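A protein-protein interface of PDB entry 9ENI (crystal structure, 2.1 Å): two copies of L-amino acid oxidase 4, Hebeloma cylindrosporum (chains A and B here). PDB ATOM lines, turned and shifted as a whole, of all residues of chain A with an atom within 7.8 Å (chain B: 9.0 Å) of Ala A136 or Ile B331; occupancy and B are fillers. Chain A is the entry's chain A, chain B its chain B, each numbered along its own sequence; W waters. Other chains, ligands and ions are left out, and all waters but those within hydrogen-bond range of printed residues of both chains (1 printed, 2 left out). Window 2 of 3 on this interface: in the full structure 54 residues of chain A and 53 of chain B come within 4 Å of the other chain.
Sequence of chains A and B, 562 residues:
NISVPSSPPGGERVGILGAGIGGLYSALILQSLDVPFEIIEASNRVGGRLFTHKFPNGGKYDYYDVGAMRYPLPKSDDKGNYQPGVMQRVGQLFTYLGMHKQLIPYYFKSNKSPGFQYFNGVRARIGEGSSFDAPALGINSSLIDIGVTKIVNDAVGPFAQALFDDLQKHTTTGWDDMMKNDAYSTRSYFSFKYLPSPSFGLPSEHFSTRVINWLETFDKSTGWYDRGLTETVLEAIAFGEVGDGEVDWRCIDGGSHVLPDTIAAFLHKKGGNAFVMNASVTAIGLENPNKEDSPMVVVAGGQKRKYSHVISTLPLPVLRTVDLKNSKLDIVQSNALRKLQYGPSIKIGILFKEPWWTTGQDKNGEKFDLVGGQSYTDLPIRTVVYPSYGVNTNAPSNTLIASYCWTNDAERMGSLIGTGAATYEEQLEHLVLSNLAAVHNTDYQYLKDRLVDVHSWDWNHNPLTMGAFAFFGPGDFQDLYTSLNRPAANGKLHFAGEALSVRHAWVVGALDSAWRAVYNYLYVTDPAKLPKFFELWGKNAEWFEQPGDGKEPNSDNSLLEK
OD1 of Asn A120 sits at hydrogen-bond distance from ND2 of Asn B335, at 3.0 Å. OD1 of Asp B479 is in salt-bridge range of NE of Arg A210 (2.6 Å).
The backbone carbonyl oxygen of Ile B331 lies within hydrogen-bond range of the side-chain amide nitrogen of Asn B335 (2.8 Å). The guanidinium group (NH2) of Arg B338 is in hydrogen-bond range of the side-chain amide oxygen (OD1) of Asn B335 (3.3 Å). The backbone NH of Asn A120 lies within hydrogen-bond range of the side-chain carboxylate of Asp A378 (2.8 Å). The side-chain amide nitrogen (ND2) of Asn A120 lies within hydrogen-bond range of the backbone carbonyl oxygen (O) of Phe A132 (2.9 Å). The backbone NH of Val B332 lies within hydrogen-bond range of the side-chain carboxylate of Asp B330 (2.9 Å). OG of Ser B334 is in hydrogen-bond range of O of Ile B331, at 3.1 Å.
CD1 of Ile B331 touches CG of Asn A120 (3.5 Å). Ile B331 touches Asp A133. Ala A136 touches Ile B331 (O to CG2, 3.6 Å). Leu A137 touches Ile B331. CD1 of Leu A137 touches ND2 of Asn B335 (3.99 Å). Val B332 touches Arg A210 (CG1 to NH2, 3.7 Å). CD of Arg B338 touches O of Asp A378, 3.4 Å away.
Of the printed residues of chain B, Asn A120 touches Ile B331 (3.5 Å) and Asn B335 (3.0 Å). No residue of chain B comes within 4 Å of Pro A135. Ala A136 touches just one residue of chain B: Ile B331. Of chain A, only Asn A120 (3.5 Å), Asp A133 (3.3 Å), Ala A136 (3.6 Å) and Leu A137 (3.9 Å) come within 4 Å of Ile B331. Ala B336 touches none of the printed residues of chain A. Leu B337 touches none of the printed residues of chain A. Of the printed residues of chain A, Asp B479 touches Arg A210 (2.6 Å). The nearest residue of chain A that does not touch Ile B331 is Phe A132 (4.2 Å). The nearest printed residue of chain B that does not touch Asn A120 is Ser B334 (4.6 Å).
Hydrophobic or aromatic side chains of chain B within 4 Å of the printed part of chain A: Ile B331 and Val B332. Along chain B the printed residues that touch a printed residue of chain A span positions 331 to 479. Among the printed residues, Asp or Glu carboxylates within 4 Å of a Lys or Arg side-chain nitrogen of the other chain: Arg A210 with Asp B479 (2.6 Å).
No position is printed for both chains.
Water W1 lies within hydrogen-bond range of the side-chain amide oxygen of Asn A120, the side-chain hydroxyl of Ser B334 and the side-chain carboxylate of Asp A378.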
ATOM      1  N   PHE A 119     -12.120  -1.184  13.636  1.00  0.00           N
ATOM      2  CA  PHE A 119     -12.934  -1.306  14.837  1.00  0.00           C
ATOM      3  C   PHE A 119     -12.718  -2.669  15.477  1.00  0.00           C
ATOM      4  O   PHE A 119     -12.679  -3.688  14.782  1.00  0.00           O
ATOM      5  CB  PHE A 119     -14.420  -1.122  14.520  1.00  0.00           C
ATOM      6  CG  PHE A 119     -14.777   0.264  14.080  1.00  0.00           C
ATOM      7  CD1 PHE A 119     -14.543   0.671  12.777  1.00  0.00           C
ATOM      8  CD2 PHE A 119     -15.359   1.157  14.963  1.00  0.00           C
ATOM      9  CE1 PHE A 119     -14.876   1.945  12.369  1.00  0.00           C
ATOM     10  CE2 PHE A 119     -15.695   2.434  14.559  1.00  0.00           C
ATOM     11  CZ  PHE A 119     -15.456   2.829  13.264  1.00  0.00           C
ATOM     12  N   ASN A 120     -12.586  -2.679  16.806  1.00  0.00           N
ATOM     13  CA  ASN A 120     -12.418  -3.917  17.569  1.00  0.00           C
ATOM     14  C   ASN A 120     -11.233  -4.725  17.049  1.00  0.00           C
ATOM     15  O   ASN A 120     -11.273  -5.954  16.988  1.00  0.00           O
ATOM     16  CB  ASN A 120     -13.698  -4.752  17.551  1.00  0.00           C
ATOM     17  CG  ASN A 120     -14.884  -3.993  18.098  1.00  0.00           C
ATOM     18  OD1 ASN A 120     -14.803  -3.394  19.171  1.00  0.00           O
ATOM     19  ND2 ASN A 120     -15.984  -3.991  17.356  1.00  0.00           N
ATOM     20  N   GLY A 121     -10.179  -4.019  16.642  1.00  0.00           N
ATOM     21  CA  GLY A 121      -8.978  -4.648  16.142  1.00  0.00           C
ATOM     22  C   GLY A 121      -9.080  -5.214  14.745  1.00  0.00           C
ATOM     23  O   GLY A 121      -8.114  -5.831  14.276  1.00  0.00           O
ATOM     24  N   VAL A 122     -10.209  -5.030  14.066  1.00  0.00           N
ATOM     25  CA  VAL A 122     -10.420  -5.548  12.720  1.00  0.00           C
ATOM     26  C   VAL A 122     -10.332  -4.396  11.732  1.00  0.00           C
ATOM     27  O   VAL A 122     -10.987  -3.362  11.910  1.00  0.00           O
ATOM     28  CB  VAL A 122     -11.770  -6.275  12.597  1.00  0.00           C
ATOM     29  CG1 VAL A 122     -11.966  -6.787  11.179  1.00  0.00           C
ATOM     30  CG2 VAL A 122     -11.834  -7.426  13.590  1.00  0.00           C
ATOM     31  N   SER A 131     -17.976  -7.251   9.666  1.00  0.00           N
ATOM     32  CA  SER A 131     -18.757  -7.123  10.888  1.00  0.00           C
ATOM     33  C   SER A 131     -17.930  -6.614  12.060  1.00  0.00           C
ATOM     34  O   SER A 131     -18.498  -6.318  13.116  1.00  0.00           O
ATOM     35  CB  SER A 131     -19.384  -8.467  11.270  1.00  0.00           C
ATOM     36  OG  SER A 131     -18.388  -9.382  11.689  1.00  0.00           O
ATOM     37  N   PHE A 132     -16.609  -6.519  11.903  1.00  0.00           N
ATOM     38  CA  PHE A 132     -15.731  -5.996  12.949  1.00  0.00           C
ATOM     39  C   PHE A 132     -15.944  -6.729  14.267  1.00  0.00           C
ATOM     40  O   PHE A 132     -16.042  -6.123  15.337  1.00  0.00           O
ATOM     41  CB  PHE A 132     -15.934  -4.492  13.123  1.00  0.00           C
ATOM     42  CG  PHE A 132     -15.766  -3.718  11.852  1.00  0.00           C
ATOM     43  CD1 PHE A 132     -14.501  -3.421  11.371  1.00  0.00           C
ATOM     44  CD2 PHE A 132     -16.869  -3.293  11.133  1.00  0.00           C
ATOM     45  CE1 PHE A 132     -14.342  -2.714  10.196  1.00  0.00           C
ATOM     46  CE2 PHE A 132     -16.714  -2.580   9.959  1.00  0.00           C
ATOM     47  CZ  PHE A 132     -15.451  -2.296   9.490  1.00  0.00           C
ATOM     48  N   ASP A 133     -16.031  -8.054  14.177  1.00  0.00           N
ATOM     49  CA  ASP A 133     -16.124  -8.938  15.333  1.00  0.00           C
ATOM     50  C   ASP A 133     -17.397  -8.697  16.134  1.00  0.00           C
ATOM     51  O   ASP A 133     -17.478  -9.082  17.304  1.00  0.00           O
ATOM     52  CB  ASP A 133     -14.887  -8.788  16.232  1.00  0.00           C
ATOM     53  CG  ASP A 133     -14.409 -10.115  16.813  1.00  0.00           C
ATOM     54  OD1 ASP A 133     -14.747 -11.182  16.255  1.00  0.00           O
ATOM     55  OD2 ASP A 133     -13.694 -10.093  17.838  1.00  0.00           O
ATOM     56  N   ALA A 134     -18.406  -8.087  15.524  1.00  0.00           N
ATOM     57  CA  ALA A 134     -19.652  -7.822  16.226  1.00  0.00           C
ATOM     58  C   ALA A 134     -20.283  -9.073  16.849  1.00  0.00           C
ATOM     59  O   ALA A 134     -20.913  -8.959  17.903  1.00  0.00           O
ATOM     60  CB  ALA A 134     -20.652  -7.132  15.292  1.00  0.00           C
ATOM     61  N   PRO A 135     -20.176 -10.264  16.236  1.00  0.00           N
ATOM     62  CA  PRO A 135     -20.702 -11.464  16.919  1.00  0.00           C
ATOM     63  C   PRO A 135     -20.129 -11.653  18.315  1.00  0.00           C
ATOM     64  O   PRO A 135     -20.862 -12.037  19.237  1.00  0.00           O
ATOM     65  CB  PRO A 135     -20.308 -12.605  15.972  1.00  0.00           C
ATOM     66  CG  PRO A 135     -20.242 -11.966  14.630  1.00  0.00           C
ATOM     67  CD  PRO A 135     -19.720 -10.572  14.869  1.00  0.00           C
ATOM     68  N   ALA A 136     -18.827 -11.410  18.491  1.00  0.00           N
ATOM     69  CA  ALA A 136     -18.232 -11.519  19.818  1.00  0.00           C
ATOM     70  C   ALA A 136     -18.807 -10.477  20.764  1.00  0.00           C
ATOM     71  O   ALA A 136     -18.822 -10.677  21.984  1.00  0.00           O
ATOM     72  CB  ALA A 136     -16.715 -11.367  19.723  1.00  0.00           C
ATOM     73  N   LEU A 137     -19.288  -9.365  20.219  1.00  0.00           N
ATOM     74  CA  LEU A 137     -19.901  -8.314  21.015  1.00  0.00           C
ATOM     75  C   LEU A 137     -21.338  -8.640  21.396  1.00  0.00           C
ATOM     76  O   LEU A 137     -21.941  -7.895  22.174  1.00  0.00           O
ATOM     77  CB  LEU A 137     -19.828  -6.999  20.233  1.00  0.00           C
ATOM     78  CG  LEU A 137     -20.124  -5.677  20.939  1.00  0.00           C
ATOM     79  CD1 LEU A 137     -19.238  -5.484  22.164  1.00  0.00           C
ATOM     80  CD2 LEU A 137     -19.940  -4.522  19.957  1.00  0.00           C
ATOM     81  N   GLY A 138     -21.901  -9.723  20.867  1.00  0.00           N
ATOM     82  CA  GLY A 138     -23.265 -10.092  21.180  1.00  0.00           C
ATOM     83  C   GLY A 138     -24.302  -9.577  20.211  1.00  0.00           C
ATOM     84  O   GLY A 138     -25.493  -9.576  20.545  1.00  0.00           O
ATOM     85  N   ILE A 139     -23.894  -9.126  19.032  1.00  0.00           N
ATOM     86  CA  ILE A 139     -24.824  -8.657  18.012  1.00  0.00           C
ATOM     87  C   ILE A 139     -25.182  -9.853  17.140  1.00  0.00           C
ATOM     88  O   ILE A 139     -24.313 -10.423  16.472  1.00  0.00           O
ATOM     89  CB  ILE A 139     -24.208  -7.528  17.172  1.00  0.00           C
ATOM     90  CG1 ILE A 139     -23.587  -6.447  18.068  1.00  0.00           C
ATOM     91  CG2 ILE A 139     -25.257  -6.923  16.252  1.00  0.00           C
ATOM     92  CD1 ILE A 139     -24.566  -5.791  19.015  1.00  0.00           C
ATOM     93  N   ILE A 144     -26.693  -7.811  12.169  1.00  0.00           N
ATOM     94  CA  ILE A 144     -25.515  -7.581  11.339  1.00  0.00           C
ATOM     95  C   ILE A 144     -25.902  -7.537   9.867  1.00  0.00           C
ATOM     96  O   ILE A 144     -25.464  -6.652   9.123  1.00  0.00           O
ATOM     97  CB  ILE A 144     -24.449  -8.657  11.620  1.00  0.00           C
ATOM     98  CG1 ILE A 144     -23.896  -8.477  13.036  1.00  0.00           C
ATOM     99  CG2 ILE A 144     -23.341  -8.614  10.568  1.00  0.00           C
ATOM    100  CD1 ILE A 144     -22.979  -9.602  13.490  1.00  0.00           C
ATOM    101  N   ARG A 210     -26.715  -2.852  24.499  1.00  0.00           N
ATOM    102  CA  ARG A 210     -25.572  -3.360  23.747  1.00  0.00           C
ATOM    103  C   ARG A 210     -25.723  -3.051  22.264  1.00  0.00           C
ATOM    104  O   ARG A 210     -24.782  -2.583  21.614  1.00  0.00           O
ATOM    105  CB  ARG A 210     -25.429  -4.865  23.977  1.00  0.00           C
ATOM    106  CG  ARG A 210     -24.338  -5.544  23.154  1.00  0.00           C
ATOM    107  CD  ARG A 210     -22.954  -5.017  23.501  1.00  0.00           C
ATOM    108  NE  ARG A 210     -22.655  -5.153  24.921  1.00  0.00           N
ATOM    109  CZ  ARG A 210     -22.137  -6.236  25.482  1.00  0.00           C
ATOM    110  NH1 ARG A 210     -21.852  -7.315  24.772  1.00  0.00           N
ATOM    111  NH2 ARG A 210     -21.904  -6.241  26.790  1.00  0.00           N
ATOM    112  N   ASP A 378     -12.532   3.193  16.009  1.00  0.00           N
ATOM    113  CA  ASP A 378     -12.893   3.383  17.409  1.00  0.00           C
ATOM    114  C   ASP A 378     -11.696   3.795  18.257  1.00  0.00           C
ATOM    115  O   ASP A 378     -11.852   4.001  19.465  1.00  0.00           O
ATOM    116  CB  ASP A 378     -13.542   2.117  17.989  1.00  0.00           C
ATOM    117  CG  ASP A 378     -12.702   0.871  17.791  1.00  0.00           C
ATOM    118  OD1 ASP A 378     -11.536   0.991  17.360  1.00  0.00           O
ATOM    119  OD2 ASP A 378     -13.215  -0.237  18.064  1.00  0.00           O
ATOM    120  N   LYS B 328      -4.655  -8.256  25.823  1.00  0.00           N
ATOM    121  CA  LYS B 328      -5.722  -9.186  25.464  1.00  0.00           C
ATOM    122  C   LYS B 328      -7.048  -8.809  26.124  1.00  0.00           C
ATOM    123  O   LYS B 328      -7.738  -9.641  26.716  1.00  0.00           O
ATOM    124  CB  LYS B 328      -5.320 -10.619  25.824  1.00  0.00           C
ATOM    125  CG  LYS B 328      -4.063 -11.097  25.106  1.00  0.00           C
ATOM    126  CD  LYS B 328      -3.612 -12.478  25.575  1.00  0.00           C
ATOM    127  CE  LYS B 328      -4.576 -13.577  25.149  1.00  0.00           C
ATOM    128  NZ  LYS B 328      -4.028 -14.934  25.438  1.00  0.00           N
ATOM    129  N   LEU B 329      -7.408  -7.534  26.025  1.00  0.00           N
ATOM    130  CA  LEU B 329      -8.748  -7.132  26.422  1.00  0.00           C
ATOM    131  C   LEU B 329      -9.769  -7.802  25.513  1.00  0.00           C
ATOM    132  O   LEU B 329      -9.556  -7.920  24.302  1.00  0.00           O
ATOM    133  CB  LEU B 329      -8.899  -5.615  26.354  1.00  0.00           C
ATOM    134  CG  LEU B 329      -8.383  -4.829  27.560  1.00  0.00           C
ATOM    135  CD1 LEU B 329      -6.882  -4.989  27.717  1.00  0.00           C
ATOM    136  CD2 LEU B 329      -8.768  -3.368  27.423  1.00  0.00           C
ATOM    137  N   ASP B 330     -10.871  -8.262  26.093  1.00  0.00           N
ATOM    138  CA  ASP B 330     -11.934  -8.769  25.242  1.00  0.00           C
ATOM    139  C   ASP B 330     -12.701  -7.589  24.647  1.00  0.00           C
ATOM    140  O   ASP B 330     -12.530  -6.432  25.044  1.00  0.00           O
ATOM    141  CB  ASP B 330     -12.855  -9.731  26.003  1.00  0.00           C
ATOM    142  CG  ASP B 330     -13.667  -9.060  27.099  1.00  0.00           C
ATOM    143  OD1 ASP B 330     -14.306  -8.022  26.839  1.00  0.00           O
ATOM    144  OD2 ASP B 330     -13.687  -9.595  28.227  1.00  0.00           O
ATOM    145  N   ILE B 331     -13.546  -7.898  23.663  1.00  0.00           N
ATOM    146  CA  ILE B 331     -14.180  -6.851  22.871  1.00  0.00           C
ATOM    147  C   ILE B 331     -15.037  -5.942  23.741  1.00  0.00           C
ATOM    148  O   ILE B 331     -15.182  -4.749  23.444  1.00  0.00           O
ATOM    149  CB  ILE B 331     -14.994  -7.488  21.725  1.00  0.00           C
ATOM    150  CG1 ILE B 331     -15.501  -6.408  20.767  1.00  0.00           C
ATOM    151  CG2 ILE B 331     -16.147  -8.322  22.278  1.00  0.00           C
ATOM    152  CD1 ILE B 331     -16.022  -6.973  19.456  1.00  0.00           C
ATOM    153  N   VAL B 332     -15.609  -6.473  24.823  1.00  0.00           N
ATOM    154  CA  VAL B 332     -16.430  -5.645  25.703  1.00  0.00           C
ATOM    155  C   VAL B 332     -15.546  -4.708  26.522  1.00  0.00           C
ATOM    156  O   VAL B 332     -15.824  -3.509  26.639  1.00  0.00           O
ATOM    157  CB  VAL B 332     -17.314  -6.526  26.605  1.00  0.00           C
ATOM    158  CG1 VAL B 332     -18.269  -5.656  27.416  1.00  0.00           C
ATOM    159  CG2 VAL B 332     -18.085  -7.545  25.771  1.00  0.00           C
ATOM    160  N   GLN B 333     -14.455  -5.240  27.080  1.00  0.00           N
ATOM    161  CA  GLN B 333     -13.541  -4.412  27.858  1.00  0.00           C
ATOM    162  C   GLN B 333     -13.017  -3.240  27.034  1.00  0.00           C
ATOM    163  O   GLN B 333     -12.958  -2.108  27.526  1.00  0.00           O
ATOM    164  CB  GLN B 333     -12.382  -5.262  28.386  1.00  0.00           C
ATOM    165  CG  GLN B 333     -12.809  -6.328  29.397  1.00  0.00           C
ATOM    166  CD  GLN B 333     -11.667  -7.237  29.821  1.00  0.00           C
ATOM    167  OE1 GLN B 333     -10.851  -7.665  29.000  1.00  0.00           O
ATOM    168  NE2 GLN B 333     -11.607  -7.540  31.114  1.00  0.00           N
ATOM    169  N   SER B 334     -12.624  -3.487  25.781  1.00  0.00           N
ATOM    170  CA  SER B 334     -12.086  -2.400  24.966  1.00  0.00           C
ATOM    171  C   SER B 334     -13.171  -1.382  24.614  1.00  0.00           C
ATOM    172  O   SER B 334     -12.905  -0.175  24.575  1.00  0.00           O
ATOM    173  CB  SER B 334     -11.411  -2.960  23.709  1.00  0.00           C
ATOM    174  OG  SER B 334     -12.257  -3.827  22.975  1.00  0.00           O
ATOM    175  N   ASN B 335     -14.399  -1.843  24.365  1.00  0.00           N
ATOM    176  CA  ASN B 335     -15.512  -0.912  24.207  1.00  0.00           C
ATOM    177  C   ASN B 335     -15.736  -0.109  25.482  1.00  0.00           C
ATOM    178  O   ASN B 335     -16.006   1.096  25.430  1.00  0.00           O
ATOM    179  CB  ASN B 335     -16.782  -1.673  23.830  1.00  0.00           C
ATOM    180  CG  ASN B 335     -16.957  -1.816  22.337  1.00  0.00           C
ATOM    181  OD1 ASN B 335     -17.660  -1.025  21.711  1.00  0.00           O
ATOM    182  ND2 ASN B 335     -16.300  -2.814  21.751  1.00  0.00           N
ATOM    183  N   ALA B 336     -15.631  -0.763  26.638  1.00  0.00           N
ATOM    184  CA  ALA B 336     -15.886  -0.079  27.900  1.00  0.00           C
ATOM    185  C   ALA B 336     -14.899   1.062  28.125  1.00  0.00           C
ATOM    186  O   ALA B 336     -15.280   2.133  28.610  1.00  0.00           O
ATOM    187  CB  ALA B 336     -15.828  -1.080  29.052  1.00  0.00           C
ATOM    188  N   LEU B 337     -13.620   0.849  27.798  1.00  0.00           N
ATOM    189  CA  LEU B 337     -12.634   1.907  27.996  1.00  0.00           C
ATOM    190  C   LEU B 337     -13.023   3.185  27.259  1.00  0.00           C
ATOM    191  O   LEU B 337     -12.737   4.288  27.737  1.00  0.00           O
ATOM    192  CB  LEU B 337     -11.251   1.446  27.540  1.00  0.00           C
ATOM    193  CG  LEU B 337     -10.574   0.317  28.323  1.00  0.00           C
ATOM    194  CD1 LEU B 337      -9.170   0.093  27.764  1.00  0.00           C
ATOM    195  CD2 LEU B 337     -10.531   0.590  29.817  1.00  0.00           C
ATOM    196  N   ARG B 338     -13.653   3.059  26.091  1.00  0.00           N
ATOM    197  CA  ARG B 338     -14.035   4.213  25.286  1.00  0.00           C
ATOM    198  C   ARG B 338     -15.380   4.803  25.701  1.00  0.00           C
ATOM    199  O   ARG B 338     -15.517   6.029  25.794  1.00  0.00           O
ATOM    200  CB  ARG B 338     -14.096   3.821  23.806  1.00  0.00           C
ATOM    201  CG  ARG B 338     -14.588   4.928  22.872  1.00  0.00           C
ATOM    202  CD  ARG B 338     -14.613   4.452  21.431  1.00  0.00           C
ATOM    203  NE  ARG B 338     -15.490   3.296  21.292  1.00  0.00           N
ATOM    204  CZ  ARG B 338     -16.807   3.368  21.154  1.00  0.00           C
ATOM    205  NH1 ARG B 338     -17.437   4.534  21.124  1.00  0.00           N
ATOM    206  NH2 ARG B 338     -17.512   2.245  21.060  1.00  0.00           N
ATOM    207  N   ASP B 479     -24.559  -2.321  30.726  1.00  0.00           N
ATOM    208  CA  ASP B 479     -23.969  -2.946  29.547  1.00  0.00           C
ATOM    209  C   ASP B 479     -22.469  -3.199  29.668  1.00  0.00           C
ATOM    210  O   ASP B 479     -22.004  -4.292  29.330  1.00  0.00           O
ATOM    211  CB  ASP B 479     -24.256  -2.086  28.308  1.00  0.00           C
ATOM    212  CG  ASP B 479     -23.800  -2.749  27.018  1.00  0.00           C
ATOM    213  OD1 ASP B 479     -24.001  -3.976  26.875  1.00  0.00           O
ATOM    214  OD2 ASP B 479     -23.272  -2.041  26.135  1.00  0.00           O
ATOM    215  N   LEU B 480     -21.695  -2.211  30.131  1.00  0.00           N
ATOM    216  CA  LEU B 480     -20.244  -2.252  30.008  1.00  0.00           C
ATOM    217  C   LEU B 480     -19.486  -2.290  31.328  1.00  0.00           C
ATOM    218  O   LEU B 480     -18.315  -2.685  31.331  1.00  0.00           O
ATOM    219  CB  LEU B 480     -19.755  -1.035  29.206  1.00  0.00           C
ATOM    220  CG  LEU B 480     -20.266  -0.948  27.769  1.00  0.00           C
ATOM    221  CD1 LEU B 480     -20.090   0.461  27.200  1.00  0.00           C
ATOM    222  CD2 LEU B 480     -19.551  -1.963  26.904  1.00  0.00           C
ATOM    223  N   SER B 483     -17.680  -5.639  32.634  1.00  0.00           N
ATOM    224  CA  SER B 483     -16.573  -6.167  31.844  1.00  0.00           C
ATOM    225  C   SER B 483     -15.221  -5.802  32.442  1.00  0.00           C
ATOM    226  O   SER B 483     -14.277  -6.595  32.365  1.00  0.00           O
ATOM    227  CB  SER B 483     -16.657  -5.660  30.403  1.00  0.00           C
ATOM    228  OG  SER B 483     -16.350  -4.277  30.311  1.00  0.00           O
ATOM    229  N   LEU B 484     -15.103  -4.627  33.055  1.00  0.00           N
ATOM    230  CA  LEU B 484     -13.813  -4.190  33.574  1.00  0.00           C
ATOM    231  C   LEU B 484     -13.531  -4.695  34.983  1.00  0.00           C
ATOM    232  O   LEU B 484     -12.398  -4.552  35.457  1.00  0.00           O
ATOM    233  CB  LEU B 484     -13.709  -2.662  33.538  1.00  0.00           C
ATOM    234  CG  LEU B 484     -13.653  -2.042  32.139  1.00  0.00           C
ATOM    235  CD1 LEU B 484     -13.555  -0.524  32.237  1.00  0.00           C
ATOM    236  CD2 LEU B 484     -12.488  -2.603  31.332  1.00  0.00           C
ATOM    237  N   ARG B 486     -13.760  -7.864  35.365  1.00  0.00           N
ATOM    238  CA  ARG B 486     -12.996  -9.039  34.987  1.00  0.00           C
ATOM    239  C   ARG B 486     -11.580  -8.620  34.612  1.00  0.00           C
ATOM    240  O   ARG B 486     -11.373  -7.529  34.071  1.00  0.00           O
ATOM    241  CB  ARG B 486     -13.638  -9.750  33.799  1.00  0.00           C
ATOM    242  CG  ARG B 486     -15.063 -10.211  34.019  1.00  0.00           C
ATOM    243  CD  ARG B 486     -15.520 -11.134  32.885  1.00  0.00           C
ATOM    244  NE  ARG B 486     -15.406 -10.496  31.578  1.00  0.00           N
ATOM    245  CZ  ARG B 486     -16.366  -9.789  30.997  1.00  0.00           C
ATOM    246  NH1 ARG B 486     -17.541  -9.604  31.579  1.00  0.00           N
ATOM    247  NH2 ARG B 486     -16.139  -9.247  29.803  1.00  0.00           N
HETATM  248  O   HOH W   1     -13.016  -2.376  20.557  1.00  0.00           O
